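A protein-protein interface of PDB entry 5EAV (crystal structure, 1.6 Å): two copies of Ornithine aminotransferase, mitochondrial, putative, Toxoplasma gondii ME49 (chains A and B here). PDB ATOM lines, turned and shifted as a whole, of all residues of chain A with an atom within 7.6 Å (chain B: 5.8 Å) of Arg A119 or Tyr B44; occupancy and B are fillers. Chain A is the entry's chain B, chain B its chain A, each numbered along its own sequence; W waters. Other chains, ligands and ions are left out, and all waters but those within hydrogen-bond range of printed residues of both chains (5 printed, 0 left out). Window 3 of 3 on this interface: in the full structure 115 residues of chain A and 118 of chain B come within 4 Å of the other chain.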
ATOM      1  N   VAL A 113      21.237  22.960  16.035  1.00  0.00           N
ATOM      2  CA  VAL A 113      22.449  23.446  15.432  1.00  0.00           C
ATOM      3  C   VAL A 113      22.417  23.670  13.935  1.00  0.00           C
ATOM      4  O   VAL A 113      22.957  24.664  13.439  1.00  0.00           O
ATOM      5  CB  VAL A 113      23.584  22.428  15.750  1.00  0.00           C
ATOM      6  CG1 VAL A 113      24.918  22.879  15.203  1.00  0.00           C
ATOM      7  CG2 VAL A 113      23.725  22.281  17.241  1.00  0.00           C
ATOM      8  N   THR A 114      21.737  22.798  13.218  1.00  0.00           N
ATOM      9  CA  THR A 114      21.748  22.823  11.747  1.00  0.00           C
ATOM     10  C   THR A 114      21.188  24.093  11.176  1.00  0.00           C
ATOM     11  O   THR A 114      21.846  24.743  10.331  1.00  0.00           O
ATOM     12  CB  THR A 114      21.109  21.539  11.147  1.00  0.00           C
ATOM     13  OG1 THR A 114      21.813  20.402  11.679  1.00  0.00           O
ATOM     14  CG2 THR A 114      21.204  21.594   9.594  1.00  0.00           C
ATOM     15  N   GLY A 115      19.987  24.477  11.633  1.00  0.00           N
ATOM     16  CA  GLY A 115      19.354  25.691  11.135  1.00  0.00           C
ATOM     17  C   GLY A 115      20.208  26.923  11.441  1.00  0.00           C
ATOM     18  O   GLY A 115      20.515  27.724  10.547  1.00  0.00           O
ATOM     19  N   PRO A 116      20.583  27.095  12.720  1.00  0.00           N
ATOM     20  CA  PRO A 116      21.427  28.241  12.996  1.00  0.00           C
ATOM     21  C   PRO A 116      22.707  28.276  12.152  1.00  0.00           C
ATOM     22  O   PRO A 116      23.108  29.335  11.717  1.00  0.00           O
ATOM     23  CB  PRO A 116      21.700  28.116  14.498  1.00  0.00           C
ATOM     24  CG  PRO A 116      20.417  27.519  14.982  1.00  0.00           C
ATOM     25  CD  PRO A 116      20.109  26.467  13.973  1.00  0.00           C
ATOM     26  N   ALA A 117      23.374  27.124  11.953  1.00  0.00           N
ATOM     27  CA  ALA A 117      24.602  27.129  11.177  1.00  0.00           C
ATOM     28  C   ALA A 117      24.331  27.520   9.728  1.00  0.00           C
ATOM     29  O   ALA A 117      25.139  28.188   9.086  1.00  0.00           O
ATOM     30  CB  ALA A 117      25.274  25.770  11.203  1.00  0.00           C
ATOM     31  N   CYS A 118      23.205  27.059   9.193  1.00  0.00           N
ATOM     32  CA  CYS A 118      22.832  27.448   7.834  1.00  0.00           C
ATOM     33  C   CYS A 118      22.525  28.950   7.745  1.00  0.00           C
ATOM     34  O   CYS A 118      22.916  29.634   6.782  1.00  0.00           O
ATOM     35  CB  CYS A 118      21.658  26.653   7.312  1.00  0.00           C
ATOM     36  SG  CYS A 118      22.088  24.931   6.879  1.00  0.00           S
ATOM     37  N   ARG A 119      21.842  29.481   8.748  1.00  0.00           N
ATOM     38  CA  ARG A 119      21.574  30.930   8.750  1.00  0.00           C
ATOM     39  C   ARG A 119      22.904  31.654   8.783  1.00  0.00           C
ATOM     40  O   ARG A 119      23.118  32.641   8.079  1.00  0.00           O
ATOM     41  CB  ARG A 119      20.782  31.343   9.990  1.00  0.00           C
ATOM     42  CG  ARG A 119      20.493  32.829  10.003  1.00  0.00           C
ATOM     43  CD  ARG A 119      19.576  33.328  11.129  1.00  0.00           C
ATOM     44  NE  ARG A 119      19.408  34.765  10.917  1.00  0.00           N
ATOM     45  CZ  ARG A 119      18.380  35.516  11.314  1.00  0.00           C
ATOM     46  NH1 ARG A 119      17.363  35.010  12.009  1.00  0.00           N
ATOM     47  NH2 ARG A 119      18.378  36.799  10.997  1.00  0.00           N
ATOM     48  N   PHE A 120      23.815  31.187   9.625  1.00  0.00           N
ATOM     49  CA  PHE A 120      25.124  31.840   9.712  1.00  0.00           C
ATOM     50  C   PHE A 120      25.822  31.926   8.339  1.00  0.00           C
ATOM     51  O   PHE A 120      26.345  32.964   7.975  1.00  0.00           O
ATOM     52  CB  PHE A 120      26.000  31.055  10.668  1.00  0.00           C
ATOM     53  CG  PHE A 120      27.376  31.643  10.876  1.00  0.00           C
ATOM     54  CD1 PHE A 120      28.446  31.249  10.071  1.00  0.00           C
ATOM     55  CD2 PHE A 120      27.615  32.544  11.909  1.00  0.00           C
ATOM     56  CE1 PHE A 120      29.726  31.776  10.276  1.00  0.00           C
ATOM     57  CE2 PHE A 120      28.894  33.056  12.128  1.00  0.00           C
ATOM     58  CZ  PHE A 120      29.939  32.666  11.308  1.00  0.00           C
ATOM     59  N   MET A 121      25.847  30.810   7.602  1.00  0.00           N
ATOM     60  CA  MET A 121      26.439  30.775   6.267  1.00  0.00           C
ATOM     61  C   MET A 121      25.655  31.600   5.260  1.00  0.00           C
ATOM     62  O   MET A 121      26.218  32.301   4.420  1.00  0.00           O
ATOM     63  CB  MET A 121      26.619  29.301   5.821  1.00  0.00           C
ATOM     64  CG  MET A 121      27.649  28.557   6.670  1.00  0.00           C
ATOM     65  SD  MET A 121      27.759  26.884   5.984  1.00  0.00           S
ATOM     66  CE  MET A 121      28.197  25.961   7.441  1.00  0.00           C
ATOM     67  N   ALA A 122      24.325  31.517   5.323  1.00  0.00           N
ATOM     68  CA  ALA A 122      23.472  32.268   4.414  1.00  0.00           C
ATOM     69  C   ALA A 122      23.746  33.765   4.484  1.00  0.00           C
ATOM     70  O   ALA A 122      23.788  34.460   3.463  1.00  0.00           O
ATOM     71  CB  ALA A 122      22.005  31.990   4.754  1.00  0.00           C
ATOM     72  N   GLU A 123      23.938  34.249   5.694  1.00  0.00           N
ATOM     73  CA  GLU A 123      24.234  35.665   5.929  1.00  0.00           C
ATOM     74  C   GLU A 123      25.653  35.994   5.579  1.00  0.00           C
ATOM     75  O   GLU A 123      25.917  37.059   5.030  1.00  0.00           O
ATOM     76  CB  GLU A 123      24.010  36.029   7.394  1.00  0.00           C
ATOM     77  CG  GLU A 123      22.569  35.915   7.821  1.00  0.00           C
ATOM     78  CD  GLU A 123      22.355  36.289   9.289  1.00  0.00           C
ATOM     79  OE1 GLU A 123      23.306  36.248  10.145  1.00  0.00           O
ATOM     80  OE2 GLU A 123      21.229  36.643   9.590  1.00  0.00           O
ATOM     81  N   MET A 124      26.585  35.091   5.884  1.00  0.00           N
ATOM     82  CA  MET A 124      27.997  35.366   5.574  1.00  0.00           C
ATOM     83  C   MET A 124      28.247  35.464   4.068  1.00  0.00           C
ATOM     84  O   MET A 124      28.973  36.369   3.591  1.00  0.00           O
ATOM     85  CB  MET A 124      28.914  34.293   6.241  1.00  0.00           C
ATOM     86  CG  MET A 124      30.356  34.524   5.946  1.00  0.00           C
ATOM     87  SD  MET A 124      31.406  33.409   6.832  1.00  0.00           S
ATOM     88  CE  MET A 124      31.566  34.214   8.389  1.00  0.00           C
ATOM     89  N   PHE A 125      27.552  34.634   3.293  1.00  0.00           N
ATOM     90  CA  PHE A 125      27.765  34.584   1.843  1.00  0.00           C
ATOM     91  C   PHE A 125      26.693  35.192   1.021  1.00  0.00           C
ATOM     92  O   PHE A 125      26.903  35.390  -0.169  1.00  0.00           O
ATOM     93  CB  PHE A 125      28.059  33.138   1.418  1.00  0.00           C
ATOM     94  CG  PHE A 125      29.305  32.616   2.068  1.00  0.00           C
ATOM     95  CD1 PHE A 125      30.529  32.970   1.557  1.00  0.00           C
ATOM     96  CD2 PHE A 125      29.246  31.851   3.221  1.00  0.00           C
ATOM     97  CE1 PHE A 125      31.713  32.532   2.154  1.00  0.00           C
ATOM     98  CE2 PHE A 125      30.415  31.455   3.833  1.00  0.00           C
ATOM     99  CZ  PHE A 125      31.637  31.781   3.294  1.00  0.00           C
ATOM    100  N   GLY A 126      25.567  35.543   1.652  1.00  0.00           N
ATOM    101  CA  GLY A 126      24.458  36.241   0.959  1.00  0.00           C
ATOM    102  C   GLY A 126      23.569  35.403   0.047  1.00  0.00           C
ATOM    103  O   GLY A 126      23.295  35.775  -1.127  1.00  0.00           O
ATOM    104  N   TYR A 127      23.125  34.283   0.560  1.00  0.00           N
ATOM    105  CA  TYR A 127      22.257  33.380  -0.170  1.00  0.00           C
ATOM    106  C   TYR A 127      21.042  33.024   0.620  1.00  0.00           C
ATOM    107  O   TYR A 127      21.084  33.051   1.772  1.00  0.00           O
ATOM    108  CB  TYR A 127      23.000  32.087  -0.525  1.00  0.00           C
ATOM    109  CG  TYR A 127      24.005  32.327  -1.595  1.00  0.00           C
ATOM    110  CD1 TYR A 127      23.643  32.324  -2.883  1.00  0.00           C
ATOM    111  CD2 TYR A 127      25.341  32.527  -1.289  1.00  0.00           C
ATOM    112  CE1 TYR A 127      24.553  32.567  -3.859  1.00  0.00           C
ATOM    113  CE2 TYR A 127      26.252  32.762  -2.256  1.00  0.00           C
ATOM    114  CZ  TYR A 127      25.853  32.754  -3.547  1.00  0.00           C
ATOM    115  OH  TYR A 127      26.722  33.006  -4.531  1.00  0.00           O
ATOM    116  N   ASP A 128      19.965  32.719  -0.077  1.00  0.00           N
ATOM    117  CA  ASP A 128      18.710  32.379   0.548  1.00  0.00           C
ATOM    118  C   ASP A 128      18.711  31.010   1.271  1.00  0.00           C
ATOM    119  O   ASP A 128      18.110  30.880   2.277  1.00  0.00           O
ATOM    120  CB  ASP A 128      17.596  32.304  -0.482  1.00  0.00           C
ATOM    121  CG  ASP A 128      17.228  33.652  -1.094  1.00  0.00           C
ATOM    122  OD1 ASP A 128      17.499  34.659  -0.499  1.00  0.00           O
ATOM    123  OD2 ASP A 128      16.658  33.646  -2.163  1.00  0.00           O
ATOM    124  N   ARG A 129      19.329  30.009   0.667  1.00  0.00           N
ATOM    125  CA  ARG A 129      19.227  28.639   1.108  1.00  0.00           C
ATOM    126  C   ARG A 129      20.614  27.959   1.044  1.00  0.00           C
ATOM    127  O   ARG A 129      21.287  28.136   0.128  1.00  0.00           O
ATOM    128  CB  ARG A 129      18.338  27.827   0.203  1.00  0.00           C
ATOM    129  CG  ARG A 129      16.949  28.369  -0.013  1.00  0.00           C
ATOM    130  CD  ARG A 129      15.978  28.074   1.133  1.00  0.00           C
ATOM    131  NE  ARG A 129      14.646  28.358   0.658  1.00  0.00           N
ATOM    132  CZ  ARG A 129      13.922  29.425   0.913  1.00  0.00           C
ATOM    133  NH1 ARG A 129      14.295  30.345   1.755  1.00  0.00           N
ATOM    134  NH2 ARG A 129      12.760  29.503   0.318  1.00  0.00           N
ATOM    135  N   VAL A 130      20.889  27.120   2.023  1.00  0.00           N
ATOM    136  CA  VAL A 130      22.170  26.417   2.189  1.00  0.00           C
ATOM    137  C   VAL A 130      21.904  24.930   2.276  1.00  0.00           C
ATOM    138  O   VAL A 130      21.155  24.473   3.084  1.00  0.00           O
ATOM    139  CB  VAL A 130      22.851  26.840   3.463  1.00  0.00           C
ATOM    140  CG1 VAL A 130      24.175  26.067   3.672  1.00  0.00           C
ATOM    141  CG2 VAL A 130      23.065  28.322   3.452  1.00  0.00           C
ATOM    142  N   LEU A 131      22.475  24.197   1.348  1.00  0.00           N
ATOM    143  CA  LEU A 131      22.419  22.731   1.354  1.00  0.00           C
ATOM    144  C   LEU A 131      23.806  22.250   1.866  1.00  0.00           C
ATOM    145  O   LEU A 131      24.832  22.516   1.215  1.00  0.00           O
ATOM    146  CB  LEU A 131      22.198  22.187  -0.004  1.00  0.00           C
ATOM    147  CG  LEU A 131      22.266  20.673  -0.153  1.00  0.00           C
ATOM    148  CD1 LEU A 131      21.258  19.939   0.694  1.00  0.00           C
ATOM    149  CD2 LEU A 131      22.187  20.271  -1.608  1.00  0.00           C
ATOM    150  N   VAL A 298      26.345  23.977  -0.693  1.00  0.00           N
ATOM    151  CA  VAL A 298      25.850  24.412  -1.964  1.00  0.00           C
ATOM    152  C   VAL A 298      24.866  25.502  -1.542  1.00  0.00           C
ATOM    153  O   VAL A 298      24.029  25.269  -0.649  1.00  0.00           O
ATOM    154  CB  VAL A 298      25.092  23.314  -2.755  1.00  0.00           C
ATOM    155  CG1 VAL A 298      24.521  23.879  -4.039  1.00  0.00           C
ATOM    156  CG2 VAL A 298      26.027  22.149  -3.020  1.00  0.00           C
ATOM    157  N   GLY A 300      22.361  28.989  -2.788  1.00  0.00           N
ATOM    158  CA  GLY A 300      21.777  29.657  -3.948  1.00  0.00           C
ATOM    159  C   GLY A 300      20.456  30.296  -3.567  1.00  0.00           C
ATOM    160  O   GLY A 300      20.002  30.181  -2.431  1.00  0.00           O
ATOM    161  N   VAL A 328      31.024  26.606  11.697  1.00  0.00           N
ATOM    162  CA  VAL A 328      30.833  27.972  12.190  1.00  0.00           C
ATOM    163  C   VAL A 328      32.126  28.506  12.832  1.00  0.00           C
ATOM    164  O   VAL A 328      32.515  29.659  12.602  1.00  0.00           O
ATOM    165  CB  VAL A 328      29.624  28.070  13.133  1.00  0.00           C
ATOM    166  CG1 VAL A 328      29.563  29.423  13.819  1.00  0.00           C
ATOM    167  CG2 VAL A 328      28.372  27.796  12.315  1.00  0.00           C
ATOM    168  N   TYR B  25      26.473  32.395  18.563  1.00  0.00           N
ATOM    169  CA  TYR B  25      25.656  32.823  17.449  1.00  0.00           C
ATOM    170  C   TYR B  25      24.222  32.436  17.661  1.00  0.00           C
ATOM    171  O   TYR B  25      23.326  33.278  17.542  1.00  0.00           O
ATOM    172  CB  TYR B  25      26.178  32.255  16.133  1.00  0.00           C
ATOM    173  CG  TYR B  25      25.298  32.683  14.973  1.00  0.00           C
ATOM    174  CD1 TYR B  25      25.384  33.985  14.463  1.00  0.00           C
ATOM    175  CD2 TYR B  25      24.443  31.781  14.350  1.00  0.00           C
ATOM    176  CE1 TYR B  25      24.610  34.385  13.400  1.00  0.00           C
ATOM    177  CE2 TYR B  25      23.663  32.178  13.286  1.00  0.00           C
ATOM    178  CZ  TYR B  25      23.751  33.482  12.816  1.00  0.00           C
ATOM    179  OH  TYR B  25      22.993  33.876  11.742  1.00  0.00           O
ATOM    180  N   LEU B  29      20.291  34.596  18.219  1.00  0.00           N
ATOM    181  CA  LEU B  29      19.038  34.393  17.458  1.00  0.00           C
ATOM    182  C   LEU B  29      17.793  34.301  18.336  1.00  0.00           C
ATOM    183  O   LEU B  29      16.666  34.333  17.843  1.00  0.00           O
ATOM    184  CB  LEU B  29      19.116  33.134  16.571  1.00  0.00           C
ATOM    185  CG  LEU B  29      20.265  33.018  15.578  1.00  0.00           C
ATOM    186  CD1 LEU B  29      20.208  31.699  14.801  1.00  0.00           C
ATOM    187  CD2 LEU B  29      20.326  34.188  14.642  1.00  0.00           C
ATOM    188  N   ALA B  39      11.101  27.452  12.138  1.00  0.00           N
ATOM    189  CA  ALA B  39      11.057  28.579  11.220  1.00  0.00           C
ATOM    190  C   ALA B  39      12.453  28.918  10.706  1.00  0.00           C
ATOM    191  O   ALA B  39      12.625  29.239   9.540  1.00  0.00           O
ATOM    192  CB  ALA B  39      10.353  29.803  11.840  1.00  0.00           C
ATOM    193  N   CYS B  40      13.452  28.830  11.567  1.00  0.00           N
ATOM    194  CA  CYS B  40      14.814  29.084  11.123  1.00  0.00           C
ATOM    195  C   CYS B  40      15.177  28.067  10.032  1.00  0.00           C
ATOM    196  O   CYS B  40      15.696  28.423   8.964  1.00  0.00           O
ATOM    197  CB  CYS B  40      15.719  29.072  12.314  1.00  0.00           C
ATOM    198  SG  CYS B  40      17.495  29.173  11.951  1.00  0.00           S
ATOM    199  N   ASP B  41      14.796  26.807  10.241  1.00  0.00           N
ATOM    200  CA  ASP B  41      15.095  25.763   9.269  1.00  0.00           C
ATOM    201  C   ASP B  41      14.372  26.031   7.944  1.00  0.00           C
ATOM    202  O   ASP B  41      14.969  25.984   6.857  1.00  0.00           O
ATOM    203  CB  ASP B  41      14.772  24.372   9.847  1.00  0.00           C
ATOM    204  CG  ASP B  41      15.901  23.822  10.718  1.00  0.00           C
ATOM    205  OD1 ASP B  41      16.255  24.413  11.805  1.00  0.00           O
ATOM    206  OD2 ASP B  41      16.441  22.757  10.277  1.00  0.00           O
ATOM    207  N   ARG B  42      13.090  26.383   8.008  1.00  0.00           N
ATOM    208  CA  ARG B  42      12.393  26.687   6.777  1.00  0.00           C
ATOM    209  C   ARG B  42      12.991  27.821   5.958  1.00  0.00           C
ATOM    210  O   ARG B  42      12.952  27.792   4.726  1.00  0.00           O
ATOM    211  CB  ARG B  42      10.901  27.006   7.008  1.00  0.00           C
ATOM    212  CG  ARG B  42      10.047  25.793   7.347  1.00  0.00           C
ATOM    213  CD  ARG B  42       8.573  26.167   7.363  1.00  0.00           C
ATOM    214  NE  ARG B  42       8.260  27.115   8.442  1.00  0.00           N
ATOM    215  CZ  ARG B  42       7.866  26.788   9.684  1.00  0.00           C
ATOM    216  NH1 ARG B  42       7.766  25.527  10.067  1.00  0.00           N
ATOM    217  NH2 ARG B  42       7.612  27.744  10.568  1.00  0.00           N
ATOM    218  N   GLN B  43      13.552  28.827   6.623  1.00  0.00           N
ATOM    219  CA  GLN B  43      14.050  29.990   5.918  1.00  0.00           C
ATOM    220  C   GLN B  43      15.421  29.839   5.302  1.00  0.00           C
ATOM    221  O   GLN B  43      15.670  30.358   4.230  1.00  0.00           O
ATOM    222  CB  GLN B  43      14.103  31.189   6.888  1.00  0.00           C
ATOM    223  CG  GLN B  43      14.574  32.495   6.270  1.00  0.00           C
ATOM    224  CD  GLN B  43      13.635  32.988   5.207  1.00  0.00           C
ATOM    225  OE1 GLN B  43      13.983  33.071   4.009  1.00  0.00           O
ATOM    226  NE2 GLN B  43      12.433  33.306   5.618  1.00  0.00           N
ATOM    227  N   TYR B  44      16.297  29.166   6.012  1.00  0.00           N
ATOM    228  CA  TYR B  44      17.701  29.067   5.621  1.00  0.00           C
ATOM    229  C   TYR B  44      18.261  27.742   5.149  1.00  0.00           C
ATOM    230  O   TYR B  44      19.293  27.730   4.461  1.00  0.00           O
ATOM    231  CB  TYR B  44      18.548  29.551   6.810  1.00  0.00           C
ATOM    232  CG  TYR B  44      18.216  30.957   7.207  1.00  0.00           C
ATOM    233  CD1 TYR B  44      18.633  32.031   6.426  1.00  0.00           C
ATOM    234  CD2 TYR B  44      17.454  31.229   8.345  1.00  0.00           C
ATOM    235  CE1 TYR B  44      18.325  33.349   6.773  1.00  0.00           C
ATOM    236  CE2 TYR B  44      17.114  32.549   8.667  1.00  0.00           C
ATOM    237  CZ  TYR B  44      17.549  33.589   7.889  1.00  0.00           C
ATOM    238  OH  TYR B  44      17.188  34.901   8.242  1.00  0.00           O
ATOM    239  N   VAL B  45      17.635  26.644   5.518  1.00  0.00           N
ATOM    240  CA  VAL B  45      18.109  25.302   5.149  1.00  0.00           C
ATOM    241  C   VAL B  45      17.386  24.860   3.905  1.00  0.00           C
ATOM    242  O   VAL B  45      16.154  25.026   3.798  1.00  0.00           O
ATOM    243  CB  VAL B  45      17.816  24.301   6.282  1.00  0.00           C
ATOM    244  CG1 VAL B  45      18.383  22.927   5.989  1.00  0.00           C
ATOM    245  CG2 VAL B  45      18.390  24.780   7.604  1.00  0.00           C
ATOM    246  N   CYS B  46      18.119  24.327   2.948  1.00  0.00           N
ATOM    247  CA  CYS B  46      17.538  23.811   1.721  1.00  0.00           C
ATOM    248  C   CYS B  46      16.452  22.842   2.124  1.00  0.00           C
ATOM    249  O   CYS B  46      16.632  22.036   3.006  1.00  0.00           O
ATOM    250  CB  CYS B  46      18.647  23.172   0.896  1.00  0.00           C
ATOM    251  SG  CYS B  46      18.156  22.358  -0.619  1.00  0.00           S
HETATM  252  O   HOH W   1      19.359  36.606   8.034  1.00  0.00           O
HETATM  253  O   HOH W   2      16.918  33.181   3.510  1.00  0.00           O
HETATM  254  O   HOH W   3      16.788  32.515  13.110  1.00  0.00           O
HETATM  255  O   HOH W   4      16.231  34.462  15.115  1.00  0.00           O
HETATM  256  O   HOH W   5      18.239  23.337  13.356  1.00  0.00           O
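N of Tyr A127 sits at hydrogen-bond distance from O of Ala A122. NE of Arg A119 lies within salt-bridge range of OE2 of Glu A123, 2.9 Å away. The backbone NH (N) of Leu A131 sits at hydrogen-bond distance from the backbone carbonyl oxygen (O) of Val A298, at 2.7 Å. O of Gly A300 is in hydrogen-bond range of N of Asp A128, at 3.5 Å. The backbone carbonyl oxygen (O) of Thr A114 sits at hydrogen-bond distance from the side-chain sulfur (SG) of Cys A118, at 3.5 Å. The backbone NH (N) of Arg A129 lies within hydrogen-bond range of the backbone carbonyl oxygen (O) of Gly A300 (3.2 Å).
N of Cys B46 sits at hydrogen-bond distance from O of Val A130 (3.0 Å). The side-chain sulfur (SG) of Cys B40 lies close to the backbone carbonyl oxygen (O) of Gly A115 (3.6 Å). The backbone carbonyl oxygen (O) of Tyr B44 sits at hydrogen-bond distance from the backbone NH (N) of Val A130 (3.0 Å). NE of Arg A119 lies close to OH of Tyr B44. The backbone carbonyl oxygen (O) of Gln B43 sits at hydrogen-bond distance from the guanidinium group (NH1) of Arg A129 (2.8 Å). The backbone carbonyl oxygen (O) of Asp A128 lies close to the backbone carbonyl oxygen (O) of Gln B43 (3.2 Å). OH of Tyr B25 sits at hydrogen-bond distance from OE1 of Glu A123 (2.9 Å).
Water W1 lies within hydrogen-bond range of OE2 of Glu A123, OH of Tyr B44 and NH2 of Arg A119. Water W5 bridges N of Gly A115 (2.7 Å) and OD1 of Asp B41 (2.7 Å). Water W4 lies within hydrogen-bond range of the backbone carbonyl oxygen (O) of Leu B29 (2.8 Å) and the guanidinium group (NH1) of Arg A119 (3.4 Å). Water W3 lies within hydrogen-bond range of the guanidinium group (NH1) of Arg A119 and the side-chain sulfur (SG) of Cys B40. Water W2 bridges O of Asp A128 (2.9 Å) and OE1 of Gln B43 (3.0 Å).
No position is printed for both chains. Of the 22 pairs that touch across the chains among the printed residues, none has its exchanged pair printed and touching as well.
Gly A115 touches Asp B41. Val B45 touches Gly A115. Tyr B25 touches Pro A116. Pro A116 touches Cys B40. CB of Cys A118 touches O of Tyr B44, at 3.9 Å. Cys A118 touches Val B45. Tyr B25 touches Arg A119 (OH to CG, 3.2 Å). Leu B29 touches Arg A119 (CD2 to CD, 3.7 Å). O of Asp A128 touches CA of Tyr B44, at 3.8 Å. Arg A129 touches Tyr B44.
Arg A119 touches just these residues of chain B: Tyr B25, Leu B29 and Tyr B44. Tyr B44 touches just these residues of chain A: Cys A118 (3.9 Å), Arg A119 (3.4 Å), Ala A122 (3.8 Å), Asp A128 (3.8 Å), Arg A129 (3.5 Å) and Val A130 (3.0 Å). Printed residues of chain A within 4 Å of Leu B29: Pro A116 (3.9 Å) and Arg A119 (3.7 Å). Of the printed residues of chain A, Tyr B25 touches Pro A116 (3.3 Å), Arg A119 (3.2 Å), Phe A120 (3.5 Å) and Glu A123 (2.9 Å). Of the printed residues of chain B, Val A130 touches Tyr B44, Val B45 and Cys B46. Of the printed residues of chain A, Val B45 touches Gly A115, Cys A118 and Val A130. Val A113 touches none of the printed residues of chain B. The nearest residue of chain B that does not touch Arg A119 is Cys B40 (4.4 Å). The nearest printed residue of chain A that does not touch Tyr B44 is Gly A115 (4.6 Å).
Of the 10 printed residues of chain B, 8 touch a printed residue of chain A. Of the 22 printed residues of chain A, 11 touch a printed residue of chain B. Among the printed residues, no Asp or Glu carboxylate lies within 4 Å of a Lys or Arg side-chain nitrogen of the other chain.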
